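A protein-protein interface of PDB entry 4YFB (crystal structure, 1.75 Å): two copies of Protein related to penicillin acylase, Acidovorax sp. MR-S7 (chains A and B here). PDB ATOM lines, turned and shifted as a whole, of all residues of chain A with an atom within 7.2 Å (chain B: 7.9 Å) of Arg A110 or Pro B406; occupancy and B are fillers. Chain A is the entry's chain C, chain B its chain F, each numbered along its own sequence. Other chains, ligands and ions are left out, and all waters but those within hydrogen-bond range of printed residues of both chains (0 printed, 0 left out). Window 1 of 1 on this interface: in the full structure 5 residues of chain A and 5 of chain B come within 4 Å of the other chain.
Of chain A, only Arg A110 (3.7 Å), Asp A113 (3.4 Å) and Gly A114 (3.8 Å) come within 4 Å of Pro B406.
No residue of chain B comes within 4 Å of Ser A109.
Of the printed residues of chain A, Ala B408 touches Asp A113 (3.0 Å).
Of the printed residues of chain A, Thr B407 touches Asp A113 (3.0 Å).
Of the printed residues of chain B, Gly A114 touches Pro B406 (3.8 Å).
Of the printed residues of chain B, Asp A113 touches Pro B406, Thr B407 and Ala B408.
The nearest residue of chain B that does not touch Arg A110 is Arg B404 (4.8 Å).
The nearest printed residue of chain A that does not touch Thr B407 is Gly A114 (4.9 Å).
No position is printed for both chains.
The side-chain carboxylate (OD1) of Asp A113 lies within hydrogen-bond range of the side-chain hydroxyl (OG) of Ser A115 (2.7 Å).
Hydrophobic or aromatic side chains of chain B that line the printed part of chain A: Pro B406 and Ala B408.
Of the 11 printed residues of chain A, 3 touch a printed residue of chain B.
The backbone NH (N) of Thr B407 lies within hydrogen-bond range of the backbone carbonyl oxygen (O) of Asp A113 (3.0 Å).
O of Asp A113 lies within hydrogen-bond range of N of Ala B408, 3.0 Å away.
Among the printed residues, merely in contact across the chains: Arg A110 with Pro B406, Asp A113 with Pro B406 and Gly A114 with Pro B406.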
ATOM      1  N   VAL A 107      -9.880  12.929 -11.137  1.00  0.00           N
ATOM      2  CA  VAL A 107     -10.429  13.474 -12.398  1.00  0.00           C
ATOM      3  C   VAL A 107     -11.925  13.194 -12.433  1.00  0.00           C
ATOM      4  O   VAL A 107     -12.337  12.048 -12.329  1.00  0.00           O
ATOM      5  CB  VAL A 107      -9.757  12.831 -13.649  1.00  0.00           C
ATOM      6  CG1 VAL A 107     -10.447  13.248 -14.951  1.00  0.00           C
ATOM      7  CG2 VAL A 107      -8.265  13.179 -13.714  1.00  0.00           C
ATOM      8  N   PRO A 108     -12.750  14.244 -12.613  1.00  0.00           N
ATOM      9  CA  PRO A 108     -14.180  13.929 -12.706  1.00  0.00           C
ATOM     10  C   PRO A 108     -14.492  13.466 -14.140  1.00  0.00           C
ATOM     11  O   PRO A 108     -13.868  13.992 -15.110  1.00  0.00           O
ATOM     12  CB  PRO A 108     -14.861  15.250 -12.359  1.00  0.00           C
ATOM     13  CG  PRO A 108     -13.759  16.255 -12.143  1.00  0.00           C
ATOM     14  CD  PRO A 108     -12.463  15.678 -12.666  1.00  0.00           C
ATOM     15  N   SER A 109     -15.382  12.475 -14.254  1.00  0.00           N
ATOM     16  CA  SER A 109     -15.683  11.821 -15.513  1.00  0.00           C
ATOM     17  C   SER A 109     -17.180  11.610 -15.662  1.00  0.00           C
ATOM     18  O   SER A 109     -17.811  10.921 -14.835  1.00  0.00           O
ATOM     19  CB  SER A 109     -14.924  10.478 -15.622  1.00  0.00           C
ATOM     20  OG  SER A 109     -15.292   9.767 -16.799  1.00  0.00           O
ATOM     21  N   ARG A 110     -17.730  12.182 -16.726  1.00  0.00           N
ATOM     22  CA  ARG A 110     -19.162  12.037 -17.023  1.00  0.00           C
ATOM     23  C   ARG A 110     -19.512  10.625 -17.475  1.00  0.00           C
ATOM     24  O   ARG A 110     -18.848  10.077 -18.360  1.00  0.00           O
ATOM     25  CB  ARG A 110     -19.565  12.997 -18.139  1.00  0.00           C
ATOM     26  CG  ARG A 110     -21.076  13.167 -18.215  1.00  0.00           C
ATOM     27  CD  ARG A 110     -21.422  14.581 -18.731  1.00  0.00           C
ATOM     28  NE  ARG A 110     -22.851  14.880 -18.558  1.00  0.00           N
ATOM     29  CZ  ARG A 110     -23.751  14.512 -19.464  1.00  0.00           C
ATOM     30  NH1 ARG A 110     -23.328  13.863 -20.551  1.00  0.00           N
ATOM     31  NH2 ARG A 110     -25.048  14.777 -19.310  1.00  0.00           N
ATOM     32  N   ASN A 111     -20.577  10.071 -16.901  1.00  0.00           N
ATOM     33  CA  ASN A 111     -21.076   8.757 -17.294  1.00  0.00           C
ATOM     34  C   ASN A 111     -22.198   8.787 -18.346  1.00  0.00           C
ATOM     35  O   ASN A 111     -22.894   9.804 -18.519  1.00  0.00           O
ATOM     36  CB  ASN A 111     -21.542   7.987 -16.073  1.00  0.00           C
ATOM     37  CG  ASN A 111     -20.461   7.863 -15.033  1.00  0.00           C
ATOM     38  OD1 ASN A 111     -19.384   7.335 -15.314  1.00  0.00           O
ATOM     39  ND2 ASN A 111     -20.709   8.377 -13.856  1.00  0.00           N
ATOM     40  N   ALA A 112     -22.377   7.645 -19.023  1.00  0.00           N
ATOM     41  CA  ALA A 112     -23.536   7.421 -19.902  1.00  0.00           C
ATOM     42  C   ALA A 112     -24.851   8.001 -19.357  1.00  0.00           C
ATOM     43  O   ALA A 112     -25.597   8.606 -20.097  1.00  0.00           O
ATOM     44  CB  ALA A 112     -23.684   5.931 -20.194  1.00  0.00           C
ATOM     45  N   ASP A 113     -25.130   7.879 -18.069  1.00  0.00           N
ATOM     46  CA  ASP A 113     -26.444   8.327 -17.559  1.00  0.00           C
ATOM     47  C   ASP A 113     -26.517   9.798 -17.084  1.00  0.00           C
ATOM     48  O   ASP A 113     -27.543  10.251 -16.550  1.00  0.00           O
ATOM     49  CB  ASP A 113     -26.884   7.420 -16.431  1.00  0.00           C
ATOM     50  CG  ASP A 113     -25.978   7.510 -15.238  1.00  0.00           C
ATOM     51  OD1 ASP A 113     -24.950   8.216 -15.275  1.00  0.00           O
ATOM     52  OD2 ASP A 113     -26.283   6.842 -14.250  1.00  0.00           O
ATOM     53  N   GLY A 114     -25.397  10.511 -17.219  1.00  0.00           N
ATOM     54  CA  GLY A 114     -25.369  11.964 -16.972  1.00  0.00           C
ATOM     55  C   GLY A 114     -24.712  12.349 -15.654  1.00  0.00           C
ATOM     56  O   GLY A 114     -24.265  13.491 -15.462  1.00  0.00           O
ATOM     57  N   SER A 115     -24.621  11.386 -14.748  1.00  0.00           N
ATOM     58  CA  SER A 115     -23.952  11.624 -13.496  1.00  0.00           C
ATOM     59  C   SER A 115     -22.435  11.736 -13.768  1.00  0.00           C
ATOM     60  O   SER A 115     -21.931  11.416 -14.855  1.00  0.00           O
ATOM     61  CB  SER A 115     -24.256  10.502 -12.524  1.00  0.00           C
ATOM     62  OG  SER A 115     -23.747   9.302 -13.098  1.00  0.00           O
ATOM     63  N   VAL A 116     -21.732  12.255 -12.775  1.00  0.00           N
ATOM     64  CA  VAL A 116     -20.302  12.433 -12.826  1.00  0.00           C
ATOM     65  C   VAL A 116     -19.635  11.605 -11.711  1.00  0.00           C
ATOM     66  O   VAL A 116     -20.049  11.674 -10.540  1.00  0.00           O
ATOM     67  CB  VAL A 116     -19.945  13.923 -12.738  1.00  0.00           C
ATOM     68  CG1 VAL A 116     -18.460  14.111 -12.847  1.00  0.00           C
ATOM     69  CG2 VAL A 116     -20.575  14.695 -13.882  1.00  0.00           C
ATOM     70  N   SER A 117     -18.682  10.749 -12.081  1.00  0.00           N
ATOM     71  CA  SER A 117     -17.920   9.923 -11.127  1.00  0.00           C
ATOM     72  C   SER A 117     -16.526  10.526 -10.985  1.00  0.00           C
ATOM     73  O   SER A 117     -15.920  10.897 -11.987  1.00  0.00           O
ATOM     74  CB  SER A 117     -17.755   8.503 -11.676  1.00  0.00           C
ATOM     75  OG  SER A 117     -19.005   7.821 -11.691  1.00  0.00           O
ATOM     76  N   PHE B 401     -31.305  14.254 -29.741  1.00  0.00           N
ATOM     77  CA  PHE B 401     -31.705  14.753 -28.432  1.00  0.00           C
ATOM     78  C   PHE B 401     -31.781  13.610 -27.396  1.00  0.00           C
ATOM     79  O   PHE B 401     -31.114  13.640 -26.391  1.00  0.00           O
ATOM     80  CB  PHE B 401     -33.086  15.463 -28.566  1.00  0.00           C
ATOM     81  CG  PHE B 401     -33.779  15.691 -27.240  1.00  0.00           C
ATOM     82  CD1 PHE B 401     -33.236  16.554 -26.307  1.00  0.00           C
ATOM     83  CD2 PHE B 401     -34.997  15.015 -26.949  1.00  0.00           C
ATOM     84  CE1 PHE B 401     -33.891  16.816 -25.076  1.00  0.00           C
ATOM     85  CE2 PHE B 401     -35.660  15.250 -25.727  1.00  0.00           C
ATOM     86  CZ  PHE B 401     -35.092  16.127 -24.798  1.00  0.00           C
ATOM     87  N   TRP B 402     -32.660  12.628 -27.614  1.00  0.00           N
ATOM     88  CA  TRP B 402     -32.906  11.596 -26.607  1.00  0.00           C
ATOM     89  C   TRP B 402     -31.671  10.819 -26.250  1.00  0.00           C
ATOM     90  O   TRP B 402     -31.475  10.415 -25.074  1.00  0.00           O
ATOM     91  CB  TRP B 402     -34.027  10.646 -27.117  1.00  0.00           C
ATOM     92  CG  TRP B 402     -34.446   9.724 -25.989  1.00  0.00           C
ATOM     93  CD1 TRP B 402     -34.053   8.406 -25.729  1.00  0.00           C
ATOM     94  CD2 TRP B 402     -35.271  10.120 -24.880  1.00  0.00           C
ATOM     95  NE1 TRP B 402     -34.654   7.957 -24.525  1.00  0.00           N
ATOM     96  CE2 TRP B 402     -35.396   8.940 -23.988  1.00  0.00           C
ATOM     97  CE3 TRP B 402     -35.959  11.306 -24.554  1.00  0.00           C
ATOM     98  CZ2 TRP B 402     -36.122   9.005 -22.788  1.00  0.00           C
ATOM     99  CZ3 TRP B 402     -36.698  11.358 -23.344  1.00  0.00           C
ATOM    100  CH2 TRP B 402     -36.765  10.228 -22.471  1.00  0.00           C
ATOM    101  N   SER B 403     -30.792  10.571 -27.238  1.00  0.00           N
ATOM    102  CA  SER B 403     -29.585   9.795 -26.976  1.00  0.00           C
ATOM    103  C   SER B 403     -28.668  10.574 -26.033  1.00  0.00           C
ATOM    104  O   SER B 403     -27.749  10.018 -25.426  1.00  0.00           O
ATOM    105  CB  SER B 403     -28.882   9.471 -28.315  1.00  0.00           C
ATOM    106  OG  SER B 403     -28.456  10.721 -28.874  1.00  0.00           O
ATOM    107  N   ARG B 404     -28.939  11.868 -25.850  1.00  0.00           N
ATOM    108  CA  ARG B 404     -28.127  12.673 -24.942  1.00  0.00           C
ATOM    109  C   ARG B 404     -28.782  13.025 -23.601  1.00  0.00           C
ATOM    110  O   ARG B 404     -28.174  13.737 -22.797  1.00  0.00           O
ATOM    111  CB  ARG B 404     -27.712  13.995 -25.646  1.00  0.00           C
ATOM    112  CG  ARG B 404     -26.720  13.710 -26.750  1.00  0.00           C
ATOM    113  CD  ARG B 404     -26.237  15.012 -27.378  1.00  0.00           C
ATOM    114  NE  ARG B 404     -25.069  14.710 -28.236  1.00  0.00           N
ATOM    115  CZ  ARG B 404     -25.136  14.289 -29.511  1.00  0.00           C
ATOM    116  NH1 ARG B 404     -23.975  14.096 -30.179  1.00  0.00           N
ATOM    117  NH2 ARG B 404     -26.312  14.094 -30.141  1.00  0.00           N
ATOM    118  N   VAL B 405     -30.009  12.571 -23.366  1.00  0.00           N
ATOM    119  CA  VAL B 405     -30.722  13.010 -22.163  1.00  0.00           C
ATOM    120  C   VAL B 405     -30.144  12.221 -20.982  1.00  0.00           C
ATOM    121  O   VAL B 405     -30.024  11.025 -21.081  1.00  0.00           O
ATOM    122  CB  VAL B 405     -32.210  12.756 -22.306  1.00  0.00           C
ATOM    123  CG1 VAL B 405     -32.855  12.899 -20.946  1.00  0.00           C
ATOM    124  CG2 VAL B 405     -32.814  13.764 -23.319  1.00  0.00           C
ATOM    125  N   PRO B 406     -29.743  12.890 -19.900  1.00  0.00           N
ATOM    126  CA  PRO B 406     -29.229  12.174 -18.730  1.00  0.00           C
ATOM    127  C   PRO B 406     -30.349  11.368 -18.045  1.00  0.00           C
ATOM    128  O   PRO B 406     -31.305  11.939 -17.558  1.00  0.00           O
ATOM    129  CB  PRO B 406     -28.782  13.290 -17.794  1.00  0.00           C
ATOM    130  CG  PRO B 406     -28.627  14.499 -18.640  1.00  0.00           C
ATOM    131  CD  PRO B 406     -29.588  14.356 -19.785  1.00  0.00           C
ATOM    132  N   THR B 407     -30.215  10.056 -18.002  1.00  0.00           N
ATOM    133  CA  THR B 407     -31.289   9.251 -17.419  1.00  0.00           C
ATOM    134  C   THR B 407     -31.261   9.182 -15.873  1.00  0.00           C
ATOM    135  O   THR B 407     -32.266   8.829 -15.274  1.00  0.00           O
ATOM    136  CB  THR B 407     -31.328   7.866 -18.024  1.00  0.00           C
ATOM    137  OG1 THR B 407     -30.026   7.308 -17.895  1.00  0.00           O
ATOM    138  CG2 THR B 407     -31.773   7.898 -19.542  1.00  0.00           C
ATOM    139  N   ALA B 408     -30.167   9.532 -15.221  1.00  0.00           N
ATOM    140  CA  ALA B 408     -30.156   9.627 -13.762  1.00  0.00           C
ATOM    141  C   ALA B 408     -31.162  10.691 -13.347  1.00  0.00           C
ATOM    142  O   ALA B 408     -31.098  11.819 -13.840  1.00  0.00           O
ATOM    143  CB  ALA B 408     -28.795  10.056 -13.306  1.00  0.00           C
ATOM    144  N   SER B 409     -32.098  10.400 -12.462  1.00  0.00           N
ATOM    145  CA  SER B 409     -33.021  11.512 -12.100  1.00  0.00           C
ATOM    146  C   SER B 409     -33.880  12.116 -13.232  1.00  0.00           C
ATOM    147  O   SER B 409     -34.401  13.230 -13.116  1.00  0.00           O
ATOM    148  CB  SER B 409     -32.243  12.657 -11.425  1.00  0.00           C
ATOM    149  OG  SER B 409     -32.017  12.307 -10.074  1.00  0.00           O
ATOM    150  N   LEU B 410     -34.039  11.376 -14.323  1.00  0.00           N
ATOM    151  CA  LEU B 410     -34.955  11.770 -15.368  1.00  0.00           C
ATOM    152  C   LEU B 410     -36.446  11.518 -15.056  1.00  0.00           C
ATOM    153  O   LEU B 410     -37.315  12.284 -15.513  1.00  0.00           O
ATOM    154  CB  LEU B 410     -34.578  11.009 -16.639  1.00  0.00           C
ATOM    155  CG  LEU B 410     -35.359  11.336 -17.910  1.00  0.00           C
ATOM    156  CD1 LEU B 410     -35.413  12.829 -18.138  1.00  0.00           C
ATOM    157  CD2 LEU B 410     -34.817  10.547 -19.125  1.00  0.00           C
ATOM    158  N   PHE B 411     -36.720  10.409 -14.359  1.00  0.00           N
ATOM    159  CA  PHE B 411     -38.115   9.969 -14.155  1.00  0.00           C
ATOM    160  C   PHE B 411     -38.525  10.036 -12.727  1.00  0.00           C
ATOM    161  O   PHE B 411     -37.693   9.781 -11.806  1.00  0.00           O
ATOM    162  CB  PHE B 411     -38.271   8.533 -14.608  1.00  0.00           C
ATOM    163  CG  PHE B 411     -37.990   8.388 -16.089  1.00  0.00           C
ATOM    164  CD1 PHE B 411     -38.870   8.950 -17.028  1.00  0.00           C
ATOM    165  CD2 PHE B 411     -36.842   7.743 -16.510  1.00  0.00           C
ATOM    166  CE1 PHE B 411     -38.625   8.818 -18.429  1.00  0.00           C
ATOM    167  CE2 PHE B 411     -36.616   7.611 -17.875  1.00  0.00           C
ATOM    168  CZ  PHE B 411     -37.521   8.160 -18.806  1.00  0.00           C
ATOM    169  N   ALA B 431     -35.377  18.171 -14.249  1.00  0.00           N
ATOM    170  CA  ALA B 431     -34.456  17.889 -15.317  1.00  0.00           C
ATOM    171  C   ALA B 431     -34.512  18.950 -16.444  1.00  0.00           C
ATOM    172  O   ALA B 431     -33.858  18.759 -17.481  1.00  0.00           O
ATOM    173  CB  ALA B 431     -34.682  16.496 -15.888  1.00  0.00           C
ATOM    174  N   ASP B 433     -33.358  21.942 -17.059  1.00  0.00           N
ATOM    175  CA  ASP B 433     -32.087  22.528 -17.536  1.00  0.00           C
ATOM    176  C   ASP B 433     -31.312  21.518 -18.308  1.00  0.00           C
ATOM    177  O   ASP B 433     -30.757  21.832 -19.401  1.00  0.00           O
ATOM    178  CB  ASP B 433     -31.235  23.125 -16.393  1.00  0.00           C
ATOM    179  CG  ASP B 433     -31.732  24.483 -15.947  1.00  0.00           C
ATOM    180  OD1 ASP B 433     -32.617  25.114 -16.594  1.00  0.00           O
ATOM    181  OD2 ASP B 433     -31.278  24.931 -14.888  1.00  0.00           O
ATOM    182  N   ALA B 434     -31.280  20.290 -17.783  1.00  0.00           N
ATOM    183  CA  ALA B 434     -30.534  19.244 -18.447  1.00  0.00           C
ATOM    184  C   ALA B 434     -31.172  18.892 -19.799  1.00  0.00           C
ATOM    185  O   ALA B 434     -30.473  18.549 -20.785  1.00  0.00           O
ATOM    186  CB  ALA B 434     -30.428  18.005 -17.541  1.00  0.00           C
ATOM    187  N   LEU B 435     -32.508  18.950 -19.866  1.00  0.00           N
ATOM    188  CA  LEU B 435     -33.164  18.634 -21.133  1.00  0.00           C
ATOM    189  C   LEU B 435     -32.890  19.757 -22.172  1.00  0.00           C
ATOM    190  O   LEU B 435     -32.710  19.468 -23.321  1.00  0.00           O
ATOM    191  CB  LEU B 435     -34.640  18.463 -20.930  1.00  0.00           C
ATOM    192  CG  LEU B 435     -34.955  17.225 -20.087  1.00  0.00           C
ATOM    193  CD1 LEU B 435     -36.391  17.278 -19.572  1.00  0.00           C
ATOM    194  CD2 LEU B 435     -34.730  15.945 -20.878  1.00  0.00           C
ATOM    195  N   ARG B 436     -32.919  21.018 -21.724  1.00  0.00           N
ATOM    196  CA  ARG B 436     -32.547  22.103 -22.655  1.00  0.00           C
ATOM    197  C   ARG B 436     -31.102  21.980 -23.137  1.00  0.00           C
ATOM    198  O   ARG B 436     -30.831  22.312 -24.286  1.00  0.00           O
ATOM    199  CB  ARG B 436     -32.786  23.467 -21.995  1.00  0.00           C
ATOM    200  CG  ARG B 436     -34.300  23.748 -21.857  1.00  0.00           C
ATOM    201  CD  ARG B 436     -34.666  25.178 -21.428  1.00  0.00           C
ATOM    202  NE  ARG B 436     -34.480  25.224 -19.988  1.00  0.00           N
ATOM    203  CZ  ARG B 436     -35.451  25.165 -19.080  1.00  0.00           C
ATOM    204  NH1 ARG B 436     -35.084  25.111 -17.823  1.00  0.00           N
ATOM    205  NH2 ARG B 436     -36.728  25.191 -19.417  1.00  0.00           N
ATOM    206  N   GLN B 437     -30.178  21.615 -22.256  1.00  0.00           N
ATOM    207  CA  GLN B 437     -28.765  21.390 -22.693  1.00  0.00           C
ATOM    208  C   GLN B 437     -28.707  20.302 -23.780  1.00  0.00           C
ATOM    209  O   GLN B 437     -28.063  20.486 -24.816  1.00  0.00           O
ATOM    210  CB  GLN B 437     -27.914  20.950 -21.514  1.00  0.00           C
ATOM    211  CG  GLN B 437     -27.717  22.098 -20.519  1.00  0.00           C
ATOM    212  CD  GLN B 437     -27.107  21.732 -19.154  1.00  0.00           C
ATOM    213  OE1 GLN B 437     -26.477  22.579 -18.511  1.00  0.00           O
ATOM    214  NE2 GLN B 437     -27.328  20.509 -18.690  1.00  0.00           N
ATOM    215  N   ALA B 438     -29.401  19.186 -23.557  1.00  0.00           N
ATOM    216  CA  ALA B 438     -29.430  18.083 -24.567  1.00  0.00           C
ATOM    217  C   ALA B 438     -30.062  18.538 -25.867  1.00  0.00           C
ATOM    218  O   ALA B 438     -29.554  18.223 -26.965  1.00  0.00           O
ATOM    219  CB  ALA B 438     -30.191  16.815 -24.018  1.00  0.00           C
